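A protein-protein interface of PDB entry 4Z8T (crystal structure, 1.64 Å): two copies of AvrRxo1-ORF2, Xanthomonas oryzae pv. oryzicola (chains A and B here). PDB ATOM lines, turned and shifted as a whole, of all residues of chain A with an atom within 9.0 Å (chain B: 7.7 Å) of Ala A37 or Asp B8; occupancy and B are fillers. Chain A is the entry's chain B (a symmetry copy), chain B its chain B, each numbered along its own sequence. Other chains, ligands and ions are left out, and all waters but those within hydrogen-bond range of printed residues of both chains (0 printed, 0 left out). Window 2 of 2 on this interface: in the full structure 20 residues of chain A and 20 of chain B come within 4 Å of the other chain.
Ala A37 touches just these residues of chain B: Leu B4 (3.5 Å) and Asp B8 (3.5 Å).
Asp B8 touches three residues of chain A.
No residue of chain A comes within 4 Å of Gly B6.
No residue of chain A comes within 4 Å of Ala B9.
Printed residues of chain B within 4 Å of Leu A30: Phe B12 (3.8 Å).
Printed residues of chain B within 4 Å of Asp A36: Asp B8.
Of the printed residues of chain B, His A34 touches Lys B2.
Of the printed residues of chain B, Val A38 touches Lys B2 (3.5 Å).
Of the printed residues of chain B, Val A33 touches Asp B8 and Glu B11.
Gly A39 touches none of the printed residues of chain B.
The nearest residue of chain A that does not touch Asp B8 is Val A38 (5.9 Å).
Among the printed residues, merely in contact across the chains: Val A33 with Asp B8, Val A38 with Lys B2, Ala A37 with Leu B4, Ala A37 with Asp B8, Leu A30 with Phe B12 and Val A33 with Glu B11.
Of the 14 printed residues of chain A, 6 touch a printed residue of chain B.
Printed residues of chain A that touch a printed residue of chain B: Leu A30, Val A33, His A34, Asp A36, Ala A37 and Val A38.
Among the printed residues, 8 pairs touch across the chains.
Among the printed residues, no Asp or Glu carboxylate lies within 4 Å of a Lys or Arg side-chain nitrogen of the other chain.
No position is printed for both chains.
The side-chain amino group of Lys B2 sits at hydrogen-bond distance from a ring nitrogen (NE2) of His A34, at 3.5 Å.
The side-chain carboxylate of Asp A36 lies close to the side-chain carboxylate of Asp B8 (3.0 Å).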
ATOM      1  N   GLU A  29     -10.683   6.036  -7.811  1.00  0.00           N
ATOM      2  CA  GLU A  29     -11.635   6.979  -8.409  1.00  0.00           C
ATOM      3  C   GLU A  29     -12.876   6.264  -8.932  1.00  0.00           C
ATOM      4  O   GLU A  29     -14.007   6.668  -8.636  1.00  0.00           O
ATOM      5  CB  GLU A  29     -10.982   7.758  -9.545  1.00  0.00           C
ATOM      6  CG  GLU A  29      -9.881   8.698  -9.115  1.00  0.00           C
ATOM      7  CD  GLU A  29      -9.058   9.162 -10.290  1.00  0.00           C
ATOM      8  OE1 GLU A  29      -9.237   8.601 -11.403  1.00  0.00           O
ATOM      9  OE2 GLU A  29      -8.225  10.071 -10.108  1.00  0.00           O
ATOM     10  N   LEU A  30     -12.676   5.197  -9.703  1.00  0.00           N
ATOM     11  CA  LEU A  30     -13.819   4.453 -10.234  1.00  0.00           C
ATOM     12  C   LEU A  30     -14.646   3.796  -9.140  1.00  0.00           C
ATOM     13  O   LEU A  30     -15.871   3.767  -9.212  1.00  0.00           O
ATOM     14  CB  LEU A  30     -13.356   3.405 -11.252  1.00  0.00           C
ATOM     15  CG  LEU A  30     -12.728   3.987 -12.512  1.00  0.00           C
ATOM     16  CD1 LEU A  30     -12.134   2.850 -13.325  1.00  0.00           C
ATOM     17  CD2 LEU A  30     -13.786   4.729 -13.309  1.00  0.00           C
ATOM     18  N   ALA A  31     -13.969   3.268  -8.124  1.00  0.00           N
ATOM     19  CA  ALA A  31     -14.651   2.601  -7.032  1.00  0.00           C
ATOM     20  C   ALA A  31     -15.541   3.580  -6.271  1.00  0.00           C
ATOM     21  O   ALA A  31     -16.626   3.206  -5.833  1.00  0.00           O
ATOM     22  CB  ALA A  31     -13.650   1.955  -6.101  1.00  0.00           C
ATOM     23  N   LEU A  32     -15.075   4.820  -6.122  1.00  0.00           N
ATOM     24  CA  LEU A  32     -15.844   5.849  -5.414  1.00  0.00           C
ATOM     25  C   LEU A  32     -17.103   6.251  -6.170  1.00  0.00           C
ATOM     26  O   LEU A  32     -18.136   6.507  -5.556  1.00  0.00           O
ATOM     27  CB  LEU A  32     -14.993   7.087  -5.161  1.00  0.00           C
ATOM     28  CG  LEU A  32     -13.917   6.956  -4.082  1.00  0.00           C
ATOM     29  CD1 LEU A  32     -13.019   8.173  -4.087  1.00  0.00           C
ATOM     30  CD2 LEU A  32     -14.560   6.779  -2.729  1.00  0.00           C
ATOM     31  N   VAL A  33     -17.024   6.321  -7.497  1.00  0.00           N
ATOM     32  CA  VAL A  33     -18.219   6.613  -8.282  1.00  0.00           C
ATOM     33  C   VAL A  33     -19.245   5.499  -8.105  1.00  0.00           C
ATOM     34  O   VAL A  33     -20.421   5.755  -7.842  1.00  0.00           O
ATOM     35  CB  VAL A  33     -17.882   6.822  -9.774  1.00  0.00           C
ATOM     36  CG1 VAL A  33     -19.152   7.036 -10.586  1.00  0.00           C
ATOM     37  CG2 VAL A  33     -16.951   8.000  -9.931  1.00  0.00           C
ATOM     38  N   HIS A  34     -18.794   4.255  -8.230  1.00  0.00           N
ATOM     39  CA  HIS A  34     -19.670   3.111  -8.063  1.00  0.00           C
ATOM     40  C   HIS A  34     -20.258   3.060  -6.653  1.00  0.00           C
ATOM     41  O   HIS A  34     -21.428   2.716  -6.469  1.00  0.00           O
ATOM     42  CB  HIS A  34     -18.904   1.824  -8.360  1.00  0.00           C
ATOM     43  CG  HIS A  34     -19.753   0.595  -8.320  1.00  0.00           C
ATOM     44  ND1 HIS A  34     -19.792  -0.247  -7.225  1.00  0.00           N
ATOM     45  CD2 HIS A  34     -20.596   0.063  -9.233  1.00  0.00           C
ATOM     46  CE1 HIS A  34     -20.626  -1.241  -7.470  1.00  0.00           C
ATOM     47  NE2 HIS A  34     -21.128  -1.078  -8.679  1.00  0.00           N
ATOM     48  N   ALA A  35     -19.438   3.396  -5.662  1.00  0.00           N
ATOM     49  CA  ALA A  35     -19.882   3.402  -4.272  1.00  0.00           C
ATOM     50  C   ALA A  35     -21.001   4.422  -4.053  1.00  0.00           C
ATOM     51  O   ALA A  35     -22.006   4.115  -3.413  1.00  0.00           O
ATOM     52  CB  ALA A  35     -18.716   3.667  -3.336  1.00  0.00           C
ATOM     53  N   ASP A  36     -20.814   5.633  -4.572  1.00  0.00           N
ATOM     54  CA  ASP A  36     -21.850   6.666  -4.511  1.00  0.00           C
ATOM     55  C   ASP A  36     -23.133   6.167  -5.155  1.00  0.00           C
ATOM     56  O   ASP A  36     -24.230   6.351  -4.622  1.00  0.00           O
ATOM     57  CB  ASP A  36     -21.378   7.931  -5.233  1.00  0.00           C
ATOM     58  CG  ASP A  36     -22.446   9.018  -5.278  1.00  0.00           C
ATOM     59  OD1 ASP A  36     -23.317   8.983  -6.177  1.00  0.00           O
ATOM     60  OD2 ASP A  36     -22.406   9.925  -4.419  1.00  0.00           O
ATOM     61  N   ALA A  37     -22.987   5.530  -6.309  1.00  0.00           N
ATOM     62  CA  ALA A  37     -24.123   5.074  -7.093  1.00  0.00           C
ATOM     63  C   ALA A  37     -24.982   4.040  -6.371  1.00  0.00           C
ATOM     64  O   ALA A  37     -26.202   4.022  -6.540  1.00  0.00           O
ATOM     65  CB  ALA A  37     -23.643   4.519  -8.420  1.00  0.00           C
ATOM     66  N   VAL A  38     -24.352   3.177  -5.577  1.00  0.00           N
ATOM     67  CA  VAL A  38     -25.076   2.084  -4.931  1.00  0.00           C
ATOM     68  C   VAL A  38     -25.408   2.381  -3.465  1.00  0.00           C
ATOM     69  O   VAL A  38     -26.054   1.576  -2.792  1.00  0.00           O
ATOM     70  CB  VAL A  38     -24.332   0.728  -5.062  1.00  0.00           C
ATOM     71  CG1 VAL A  38     -23.879   0.512  -6.488  1.00  0.00           C
ATOM     72  CG2 VAL A  38     -23.133   0.673  -4.130  1.00  0.00           C
ATOM     73  N   GLY A  39     -24.966   3.536  -2.976  1.00  0.00           N
ATOM     74  CA  GLY A  39     -25.293   3.959  -1.625  1.00  0.00           C
ATOM     75  C   GLY A  39     -24.413   3.376  -0.536  1.00  0.00           C
ATOM     76  O   GLY A  39     -24.816   3.305   0.627  1.00  0.00           O
ATOM     77  N   LYS A  40     -23.203   2.964  -0.906  1.00  0.00           N
ATOM     78  CA  LYS A  40     -22.251   2.410   0.052  1.00  0.00           C
ATOM     79  C   LYS A  40     -21.923   3.451   1.122  1.00  0.00           C
ATOM     80  O   LYS A  40     -21.753   4.630   0.813  1.00  0.00           O
ATOM     81  CB  LYS A  40     -20.983   1.975  -0.696  1.00  0.00           C
ATOM     82  CG  LYS A  40     -19.835   1.445   0.164  1.00  0.00           C
ATOM     83  CD  LYS A  40     -18.847   0.704  -0.735  1.00  0.00           C
ATOM     84  CE  LYS A  40     -17.585   0.315   0.004  1.00  0.00           C
ATOM     85  NZ  LYS A  40     -17.132  -1.032  -0.440  1.00  0.00           N
ATOM     86  N   TYR A  75     -12.956   0.545  -0.415  1.00  0.00           N
ATOM     87  CA  TYR A  75     -13.581   0.894  -1.686  1.00  0.00           C
ATOM     88  C   TYR A  75     -13.144   0.015  -2.848  1.00  0.00           C
ATOM     89  O   TYR A  75     -13.969  -0.353  -3.675  1.00  0.00           O
ATOM     90  CB  TYR A  75     -13.314   2.350  -2.040  1.00  0.00           C
ATOM     91  CG  TYR A  75     -14.173   3.314  -1.249  1.00  0.00           C
ATOM     92  CD1 TYR A  75     -15.558   3.247  -1.320  1.00  0.00           C
ATOM     93  CD2 TYR A  75     -13.597   4.282  -0.443  1.00  0.00           C
ATOM     94  CE1 TYR A  75     -16.352   4.129  -0.599  1.00  0.00           C
ATOM     95  CE2 TYR A  75     -14.385   5.174   0.284  1.00  0.00           C
ATOM     96  CZ  TYR A  75     -15.760   5.082   0.196  1.00  0.00           C
ATOM     97  OH  TYR A  75     -16.560   5.948   0.908  1.00  0.00           O
ATOM     98  N   MET A  82     -21.124  -2.897   1.986  1.00  0.00           N
ATOM     99  CA  MET A  82     -21.872  -1.639   1.987  1.00  0.00           C
ATOM    100  C   MET A  82     -21.654  -0.776   3.232  1.00  0.00           C
ATOM    101  O   MET A  82     -21.880   0.441   3.206  1.00  0.00           O
ATOM    102  CB  MET A  82     -23.366  -1.922   1.809  1.00  0.00           C
ATOM    103  CG  MET A  82     -23.724  -2.558   0.483  1.00  0.00           C
ATOM    104  SD  MET A  82     -23.446  -1.328  -0.994  1.00  0.00           S
ATOM    105  CE  MET A  82     -22.022  -2.293  -1.905  1.00  0.00           C
ATOM    106  N   LYS B   2     -26.558  -2.691 -10.889  1.00  0.00           N
ATOM    107  CA  LYS B   2     -27.136  -1.353 -10.911  1.00  0.00           C
ATOM    108  C   LYS B   2     -26.626  -0.505 -12.083  1.00  0.00           C
ATOM    109  O   LYS B   2     -25.417  -0.376 -12.271  1.00  0.00           O
ATOM    110  CB  LYS B   2     -26.729  -0.674  -9.607  1.00  0.00           C
ATOM    111  CG  LYS B   2     -25.427  -1.247  -9.021  1.00  0.00           C
ATOM    112  CD  LYS B   2     -25.684  -2.251  -7.877  1.00  0.00           C
ATOM    113  CE  LYS B   2     -25.010  -3.607  -8.119  1.00  0.00           C
ATOM    114  NZ  LYS B   2     -23.521  -3.524  -8.128  1.00  0.00           N
ATOM    115  N   THR B   3     -27.539   0.079 -12.856  1.00  0.00           N
ATOM    116  CA  THR B   3     -27.154   0.963 -13.960  1.00  0.00           C
ATOM    117  C   THR B   3     -26.704   2.319 -13.417  1.00  0.00           C
ATOM    118  O   THR B   3     -27.415   2.924 -12.617  1.00  0.00           O
ATOM    119  CB  THR B   3     -28.334   1.199 -14.934  1.00  0.00           C
ATOM    120  OG1 THR B   3     -28.654  -0.018 -15.626  1.00  0.00           O
ATOM    121  CG2 THR B   3     -27.978   2.252 -15.956  1.00  0.00           C
ATOM    122  N   LEU B   4     -25.534   2.798 -13.846  1.00  0.00           N
ATOM    123  CA  LEU B   4     -25.098   4.161 -13.520  1.00  0.00           C
ATOM    124  C   LEU B   4     -25.818   5.133 -14.440  1.00  0.00           C
ATOM    125  O   LEU B   4     -25.868   4.919 -15.653  1.00  0.00           O
ATOM    126  CB  LEU B   4     -23.592   4.324 -13.717  1.00  0.00           C
ATOM    127  CG  LEU B   4     -22.686   3.305 -13.046  1.00  0.00           C
ATOM    128  CD1 LEU B   4     -21.225   3.637 -13.309  1.00  0.00           C
ATOM    129  CD2 LEU B   4     -22.958   3.284 -11.569  1.00  0.00           C
ATOM    130  N   THR B   5     -26.377   6.197 -13.865  1.00  0.00           N
ATOM    131  CA  THR B   5     -27.182   7.150 -14.615  1.00  0.00           C
ATOM    132  C   THR B   5     -26.666   8.547 -14.328  1.00  0.00           C
ATOM    133  O   THR B   5     -25.872   8.728 -13.397  1.00  0.00           O
ATOM    134  CB  THR B   5     -28.669   7.090 -14.192  1.00  0.00           C
ATOM    135  OG1 THR B   5     -28.791   7.526 -12.834  1.00  0.00           O
ATOM    136  CG2 THR B   5     -29.215   5.668 -14.315  1.00  0.00           C
ATOM    137  N   GLY B   6     -27.105   9.515 -15.127  1.00  0.00           N
ATOM    138  CA  GLY B   6     -26.824  10.916 -14.865  1.00  0.00           C
ATOM    139  C   GLY B   6     -25.385  11.258 -14.543  1.00  0.00           C
ATOM    140  O   GLY B   6     -24.450  10.880 -15.259  1.00  0.00           O
ATOM    141  N   ALA B   7     -25.199  11.975 -13.440  1.00  0.00           N
ATOM    142  CA  ALA B   7     -23.880  12.477 -13.097  1.00  0.00           C
ATOM    143  C   ALA B   7     -22.900  11.352 -12.815  1.00  0.00           C
ATOM    144  O   ALA B   7     -21.708  11.480 -13.129  1.00  0.00           O
ATOM    145  CB  ALA B   7     -23.972  13.411 -11.894  1.00  0.00           C
ATOM    146  N   ASP B   8     -23.386  10.261 -12.215  1.00  0.00           N
ATOM    147  CA  ASP B   8     -22.509   9.131 -11.901  1.00  0.00           C
ATOM    148  C   ASP B   8     -21.999   8.480 -13.186  1.00  0.00           C
ATOM    149  O   ASP B   8     -20.825   8.126 -13.287  1.00  0.00           O
ATOM    150  CB  ASP B   8     -23.225   8.074 -11.048  1.00  0.00           C
ATOM    151  CG  ASP B   8     -23.475   8.531  -9.620  1.00  0.00           C
ATOM    152  OD1 ASP B   8     -22.717   9.382  -9.115  1.00  0.00           O
ATOM    153  OD2 ASP B   8     -24.432   8.017  -9.003  1.00  0.00           O
ATOM    154  N   ALA B   9     -22.878   8.323 -14.172  1.00  0.00           N
ATOM    155  CA  ALA B   9     -22.449   7.737 -15.439  1.00  0.00           C
ATOM    156  C   ALA B   9     -21.402   8.626 -16.097  1.00  0.00           C
ATOM    157  O   ALA B   9     -20.374   8.143 -16.566  1.00  0.00           O
ATOM    158  CB  ALA B   9     -23.635   7.522 -16.376  1.00  0.00           C
ATOM    159  N   LEU B  10     -21.656   9.935 -16.118  1.00  0.00           N
ATOM    160  CA  LEU B  10     -20.712  10.857 -16.733  1.00  0.00           C
ATOM    161  C   LEU B  10     -19.355  10.857 -16.044  1.00  0.00           C
ATOM    162  O   LEU B  10     -18.328  10.906 -16.713  1.00  0.00           O
ATOM    163  CB  LEU B  10     -21.276  12.278 -16.784  1.00  0.00           C
ATOM    164  CG  LEU B  10     -22.335  12.530 -17.856  1.00  0.00           C
ATOM    165  CD1 LEU B  10     -22.958  13.918 -17.672  1.00  0.00           C
ATOM    166  CD2 LEU B  10     -21.736  12.400 -19.240  1.00  0.00           C
ATOM    167  N   GLU B  11     -19.355  10.810 -14.716  1.00  0.00           N
ATOM    168  CA  GLU B  11     -18.093  10.812 -13.979  1.00  0.00           C
ATOM    169  C   GLU B  11     -17.341   9.495 -14.162  1.00  0.00           C
ATOM    170  O   GLU B  11     -16.117   9.488 -14.293  1.00  0.00           O
ATOM    171  CB  GLU B  11     -18.324  11.138 -12.497  1.00  0.00           C
ATOM    172  CG  GLU B  11     -17.039  11.321 -11.673  1.00  0.00           C
ATOM    173  CD  GLU B  11     -16.264  12.596 -12.010  1.00  0.00           C
ATOM    174  OE1 GLU B  11     -16.755  13.420 -12.808  1.00  0.00           O
ATOM    175  OE2 GLU B  11     -15.149  12.776 -11.461  1.00  0.00           O
ATOM    176  N   PHE B  12     -18.065   8.377 -14.196  1.00  0.00           N
ATOM    177  CA  PHE B  12     -17.415   7.097 -14.452  1.00  0.00           C
ATOM    178  C   PHE B  12     -16.729   7.121 -15.819  1.00  0.00           C
ATOM    179  O   PHE B  12     -15.580   6.717 -15.966  1.00  0.00           O
ATOM    180  CB  PHE B  12     -18.432   5.955 -14.374  1.00  0.00           C
ATOM    181  CG  PHE B  12     -17.812   4.585 -14.283  1.00  0.00           C
ATOM    182  CD1 PHE B  12     -17.509   4.026 -13.049  1.00  0.00           C
ATOM    183  CD2 PHE B  12     -17.538   3.850 -15.429  1.00  0.00           C
ATOM    184  CE1 PHE B  12     -16.955   2.754 -12.958  1.00  0.00           C
ATOM    185  CE2 PHE B  12     -16.983   2.580 -15.337  1.00  0.00           C
ATOM    186  CZ  PHE B  12     -16.690   2.039 -14.096  1.00  0.00           C
ATOM    187  N   HIS B  13     -17.448   7.608 -16.819  1.00  0.00           N
ATOM    188  CA  HIS B  13     -16.923   7.722 -18.177  1.00  0.00           C
ATOM    189  C   HIS B  13     -15.674   8.618 -18.197  1.00  0.00           C
ATOM    190  O   HIS B  13     -14.660   8.286 -18.809  1.00  0.00           O
ATOM    191  CB  HIS B  13     -18.051   8.277 -19.064  1.00  0.00           C
ATOM    192  CG  HIS B  13     -17.682   8.467 -20.502  1.00  0.00           C
ATOM    193  ND1 HIS B  13     -17.701   7.441 -21.419  1.00  0.00           N
ATOM    194  CD2 HIS B  13     -17.348   9.586 -21.190  1.00  0.00           C
ATOM    195  CE1 HIS B  13     -17.347   7.913 -22.607  1.00  0.00           C
ATOM    196  NE2 HIS B  13     -17.136   9.207 -22.495  1.00  0.00           N
ATOM    197  N   LYS B  14     -15.748   9.759 -17.519  1.00  0.00           N
ATOM    198  CA  LYS B  14     -14.610  10.677 -17.495  1.00  0.00           C
ATOM    199  C   LYS B  14     -13.364  10.008 -16.894  1.00  0.00           C
ATOM    200  O   LYS B  14     -12.263  10.074 -17.463  1.00  0.00           O
ATOM    201  CB  LYS B  14     -14.979  11.921 -16.677  1.00  0.00           C
ATOM    202  CG  LYS B  14     -13.913  12.997 -16.675  1.00  0.00           C
ATOM    203  CD  LYS B  14     -14.425  14.189 -15.884  1.00  0.00           C
ATOM    204  CE  LYS B  14     -13.422  15.320 -15.869  1.00  0.00           C
ATOM    205  NZ  LYS B  14     -13.890  16.403 -14.944  1.00  0.00           N
